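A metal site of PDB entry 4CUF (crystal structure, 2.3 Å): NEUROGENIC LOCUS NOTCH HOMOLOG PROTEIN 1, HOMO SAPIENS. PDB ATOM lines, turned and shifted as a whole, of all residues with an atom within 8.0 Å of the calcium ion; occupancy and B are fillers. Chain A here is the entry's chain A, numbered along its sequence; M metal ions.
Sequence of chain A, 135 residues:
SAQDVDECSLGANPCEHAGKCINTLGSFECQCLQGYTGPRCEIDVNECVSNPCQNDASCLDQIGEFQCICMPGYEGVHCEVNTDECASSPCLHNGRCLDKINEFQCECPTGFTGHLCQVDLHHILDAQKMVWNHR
The calcium ion is bound by O of Gln 62 (2.3 Å), O of Val 45 (2.3 Å), OD1 of Asp 44 (2.3 Å), OD1 of Asp 61 (2.5 Å) and OE1 of Glu 47 (2.6 Å). The calcium ion has five donor atoms within binding distance.
N of Val 45 lies within hydrogen-bond range of O of Gly 35 (3.0 Å). The side-chain amide oxygen of Asn 46 sits close to the side-chain carboxylate of Asp 61, at 3.4 Å. The side-chain sulfur (SG) of Cys 48 sits at hydrogen-bond distance from the backbone NH (N) of Asp 61 (3.6 Å).
Five residues have an atom within 4 Å of the calcium ion: Asp 44, Val 45, Glu 47, Asp 61 and Gln 62. The nearest printed residue that does not touch the calcium ion is Ile 63 (4.2 Å).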
ATOM      1  N   GLN A  34     -21.055  -0.266 -20.837  1.00  0.00           N
ATOM      2  CA  GLN A  34     -19.768   0.062 -21.429  1.00  0.00           C
ATOM      3  C   GLN A  34     -18.738  -1.040 -21.192  1.00  0.00           C
ATOM      4  O   GLN A  34     -18.539  -1.514 -20.074  1.00  0.00           O
ATOM      5  CB  GLN A  34     -19.269   1.420 -20.956  1.00  0.00           C
ATOM      6  CG  GLN A  34     -18.078   1.935 -21.771  1.00  0.00           C
ATOM      7  CD  GLN A  34     -18.090   3.411 -22.043  1.00  0.00           C
ATOM      8  OE1 GLN A  34     -19.116   4.094 -21.919  1.00  0.00           O
ATOM      9  NE2 GLN A  34     -16.953   3.916 -22.484  1.00  0.00           N
ATOM     10  N   GLY A  35     -18.127  -1.428 -22.304  1.00  0.00           N
ATOM     11  CA  GLY A  35     -17.133  -2.472 -22.344  1.00  0.00           C
ATOM     12  C   GLY A  35     -17.664  -3.807 -22.795  1.00  0.00           C
ATOM     13  O   GLY A  35     -16.872  -4.747 -22.935  1.00  0.00           O
ATOM     14  N   TYR A  36     -18.993  -3.935 -23.046  1.00  0.00           N
ATOM     15  CA  TYR A  36     -19.567  -5.203 -23.472  1.00  0.00           C
ATOM     16  C   TYR A  36     -20.272  -5.129 -24.830  1.00  0.00           C
ATOM     17  O   TYR A  36     -20.766  -4.062 -25.178  1.00  0.00           O
ATOM     18  CB  TYR A  36     -20.472  -5.794 -22.373  1.00  0.00           C
ATOM     19  CG  TYR A  36     -19.692  -6.073 -21.103  1.00  0.00           C
ATOM     20  CD1 TYR A  36     -18.863  -7.190 -21.000  1.00  0.00           C
ATOM     21  CD2 TYR A  36     -19.739  -5.190 -20.018  1.00  0.00           C
ATOM     22  CE1 TYR A  36     -18.101  -7.428 -19.857  1.00  0.00           C
ATOM     23  CE2 TYR A  36     -19.019  -5.456 -18.844  1.00  0.00           C
ATOM     24  CZ  TYR A  36     -18.206  -6.587 -18.769  1.00  0.00           C
ATOM     25  OH  TYR A  36     -17.501  -6.917 -17.628  1.00  0.00           O
ATOM     26  N   ILE A  43     -19.667 -10.664 -24.875  1.00  0.00           N
ATOM     27  CA  ILE A  43     -18.279 -10.322 -25.155  1.00  0.00           C
ATOM     28  C   ILE A  43     -17.719  -9.125 -24.448  1.00  0.00           C
ATOM     29  O   ILE A  43     -18.289  -8.042 -24.495  1.00  0.00           O
ATOM     30  CB  ILE A  43     -18.005 -10.264 -26.668  1.00  0.00           C
ATOM     31  CG1 ILE A  43     -18.620 -11.485 -27.399  1.00  0.00           C
ATOM     32  CG2 ILE A  43     -16.498 -10.128 -26.967  1.00  0.00           C
ATOM     33  CD1 ILE A  43     -18.872 -11.269 -28.876  1.00  0.00           C
ATOM     34  N   ASP A  44     -16.556  -9.334 -23.863  1.00  0.00           N
ATOM     35  CA  ASP A  44     -15.795  -8.282 -23.243  1.00  0.00           C
ATOM     36  C   ASP A  44     -14.945  -7.644 -24.372  1.00  0.00           C
ATOM     37  O   ASP A  44     -13.983  -8.254 -24.851  1.00  0.00           O
ATOM     38  CB  ASP A  44     -14.921  -8.901 -22.134  1.00  0.00           C
ATOM     39  CG  ASP A  44     -13.887  -7.984 -21.509  1.00  0.00           C
ATOM     40  OD1 ASP A  44     -13.738  -6.827 -21.982  1.00  0.00           O
ATOM     41  OD2 ASP A  44     -13.195  -8.423 -20.557  1.00  0.00           O
ATOM     42  N   VAL A  45     -15.316  -6.437 -24.801  1.00  0.00           N
ATOM     43  CA  VAL A  45     -14.602  -5.651 -25.822  1.00  0.00           C
ATOM     44  C   VAL A  45     -13.117  -5.531 -25.474  1.00  0.00           C
ATOM     45  O   VAL A  45     -12.754  -5.291 -24.331  1.00  0.00           O
ATOM     46  CB  VAL A  45     -15.206  -4.233 -25.999  1.00  0.00           C
ATOM     47  CG1 VAL A  45     -14.390  -3.361 -26.961  1.00  0.00           C
ATOM     48  CG2 VAL A  45     -16.643  -4.313 -26.466  1.00  0.00           C
ATOM     49  N   ASN A  46     -12.273  -5.686 -26.500  1.00  0.00           N
ATOM     50  CA  ASN A  46     -10.844  -5.489 -26.413  1.00  0.00           C
ATOM     51  C   ASN A  46     -10.526  -4.010 -26.745  1.00  0.00           C
ATOM     52  O   ASN A  46     -10.400  -3.640 -27.924  1.00  0.00           O
ATOM     53  CB  ASN A  46     -10.087  -6.453 -27.349  1.00  0.00           C
ATOM     54  CG  ASN A  46      -8.594  -6.249 -27.322  1.00  0.00           C
ATOM     55  OD1 ASN A  46      -8.045  -5.527 -26.483  1.00  0.00           O
ATOM     56  ND2 ASN A  46      -7.903  -6.883 -28.253  1.00  0.00           N
ATOM     57  N   GLU A  47     -10.370  -3.181 -25.708  1.00  0.00           N
ATOM     58  CA  GLU A  47     -10.096  -1.752 -25.904  1.00  0.00           C
ATOM     59  C   GLU A  47      -8.701  -1.468 -26.455  1.00  0.00           C
ATOM     60  O   GLU A  47      -8.419  -0.337 -26.800  1.00  0.00           O
ATOM     61  CB  GLU A  47     -10.349  -0.953 -24.614  1.00  0.00           C
ATOM     62  CG  GLU A  47     -11.808  -0.694 -24.325  1.00  0.00           C
ATOM     63  CD  GLU A  47     -12.519  -1.856 -23.663  1.00  0.00           C
ATOM     64  OE1 GLU A  47     -11.826  -2.809 -23.230  1.00  0.00           O
ATOM     65  OE2 GLU A  47     -13.765  -1.812 -23.577  1.00  0.00           O
ATOM     66  N   CYS A  48      -7.872  -2.511 -26.570  1.00  0.00           N
ATOM     67  CA  CYS A  48      -6.514  -2.430 -27.097  1.00  0.00           C
ATOM     68  C   CYS A  48      -6.417  -2.750 -28.582  1.00  0.00           C
ATOM     69  O   CYS A  48      -5.368  -2.549 -29.173  1.00  0.00           O
ATOM     70  CB  CYS A  48      -5.597  -3.325 -26.276  1.00  0.00           C
ATOM     71  SG  CYS A  48      -5.366  -2.745 -24.585  1.00  0.00           S
ATOM     72  N   LEU A  60      -3.204  -2.521 -21.577  1.00  0.00           N
ATOM     73  CA  LEU A  60      -3.980  -3.432 -20.718  1.00  0.00           C
ATOM     74  C   LEU A  60      -5.438  -3.326 -21.073  1.00  0.00           C
ATOM     75  O   LEU A  60      -6.040  -2.250 -20.963  1.00  0.00           O
ATOM     76  CB  LEU A  60      -3.843  -3.164 -19.206  1.00  0.00           C
ATOM     77  CG  LEU A  60      -2.436  -3.070 -18.629  1.00  0.00           C
ATOM     78  CD1 LEU A  60      -2.500  -2.633 -17.157  1.00  0.00           C
ATOM     79  CD2 LEU A  60      -1.609  -4.366 -18.852  1.00  0.00           C
ATOM     80  N   ASP A  61      -6.020  -4.436 -21.489  1.00  0.00           N
ATOM     81  CA  ASP A  61      -7.408  -4.527 -21.869  1.00  0.00           C
ATOM     82  C   ASP A  61      -8.228  -4.783 -20.611  1.00  0.00           C
ATOM     83  O   ASP A  61      -8.143  -5.875 -20.054  1.00  0.00           O
ATOM     84  CB  ASP A  61      -7.579  -5.630 -22.917  1.00  0.00           C
ATOM     85  CG  ASP A  61      -9.030  -5.988 -23.257  1.00  0.00           C
ATOM     86  OD1 ASP A  61      -9.926  -5.137 -23.023  1.00  0.00           O
ATOM     87  OD2 ASP A  61      -9.263  -7.113 -23.771  1.00  0.00           O
ATOM     88  N   GLN A  62      -9.006  -3.785 -20.170  1.00  0.00           N
ATOM     89  CA  GLN A  62      -9.823  -3.833 -18.947  1.00  0.00           C
ATOM     90  C   GLN A  62     -11.305  -3.677 -19.220  1.00  0.00           C
ATOM     91  O   GLN A  62     -11.676  -3.615 -20.389  1.00  0.00           O
ATOM     92  CB  GLN A  62      -9.347  -2.768 -17.975  1.00  0.00           C
ATOM     93  CG  GLN A  62      -7.836  -2.841 -17.745  1.00  0.00           C
ATOM     94  CD  GLN A  62      -7.333  -1.639 -17.008  1.00  0.00           C
ATOM     95  OE1 GLN A  62      -7.950  -0.552 -17.017  1.00  0.00           O
ATOM     96  NE2 GLN A  62      -6.213  -1.807 -16.342  1.00  0.00           N
ATOM     97  N   ILE A  63     -12.155  -3.626 -18.181  1.00  0.00           N
ATOM     98  CA  ILE A  63     -13.616  -3.519 -18.369  1.00  0.00           C
ATOM     99  C   ILE A  63     -14.020  -2.122 -18.775  1.00  0.00           C
ATOM    100  O   ILE A  63     -13.953  -1.218 -17.944  1.00  0.00           O
ATOM    101  CB  ILE A  63     -14.430  -4.021 -17.148  1.00  0.00           C
ATOM    102  CG1 ILE A  63     -14.020  -5.455 -16.742  1.00  0.00           C
ATOM    103  CG2 ILE A  63     -15.940  -3.878 -17.386  1.00  0.00           C
ATOM    104  CD1 ILE A  63     -14.422  -5.875 -15.378  1.00  0.00           C
ATOM    105  N   GLY A  64     -14.410  -1.946 -20.027  1.00  0.00           N
ATOM    106  CA  GLY A  64     -14.806  -0.637 -20.544  1.00  0.00           C
ATOM    107  C   GLY A  64     -13.698   0.399 -20.661  1.00  0.00           C
ATOM    108  O   GLY A  64     -13.990   1.596 -20.797  1.00  0.00           O
ATOM    109  N   GLU A  65     -12.433  -0.045 -20.627  1.00  0.00           N
ATOM    110  CA  GLU A  65     -11.289   0.842 -20.768  1.00  0.00           C
ATOM    111  C   GLU A  65     -10.002   0.098 -21.041  1.00  0.00           C
ATOM    112  O   GLU A  65      -9.888  -1.120 -20.883  1.00  0.00           O
ATOM    113  CB  GLU A  65     -11.109   1.731 -19.501  1.00  0.00           C
ATOM    114  CG  GLU A  65     -10.758   0.975 -18.230  1.00  0.00           C
ATOM    115  CD  GLU A  65     -10.770   1.827 -16.983  1.00  0.00           C
ATOM    116  OE1 GLU A  65     -10.005   2.812 -16.922  1.00  0.00           O
ATOM    117  OE2 GLU A  65     -11.578   1.530 -16.071  1.00  0.00           O
ATOM    118  N   PHE A  66      -9.016   0.855 -21.440  1.00  0.00           N
ATOM    119  CA  PHE A  66      -7.661   0.365 -21.562  1.00  0.00           C
ATOM    120  C   PHE A  66      -6.797   1.190 -20.638  1.00  0.00           C
ATOM    121  O   PHE A  66      -7.147   2.290 -20.260  1.00  0.00           O
ATOM    122  CB  PHE A  66      -7.142   0.442 -23.010  1.00  0.00           C
ATOM    123  CG  PHE A  66      -7.072   1.842 -23.548  1.00  0.00           C
ATOM    124  CD1 PHE A  66      -8.182   2.413 -24.187  1.00  0.00           C
ATOM    125  CD2 PHE A  66      -5.933   2.615 -23.398  1.00  0.00           C
ATOM    126  CE1 PHE A  66      -8.134   3.717 -24.657  1.00  0.00           C
ATOM    127  CE2 PHE A  66      -5.899   3.924 -23.849  1.00  0.00           C
ATOM    128  CZ  PHE A  66      -6.980   4.457 -24.505  1.00  0.00           C
HETATM  129 CA    CA M   1     -12.223  -5.057 -22.090  1.00  0.00          CA
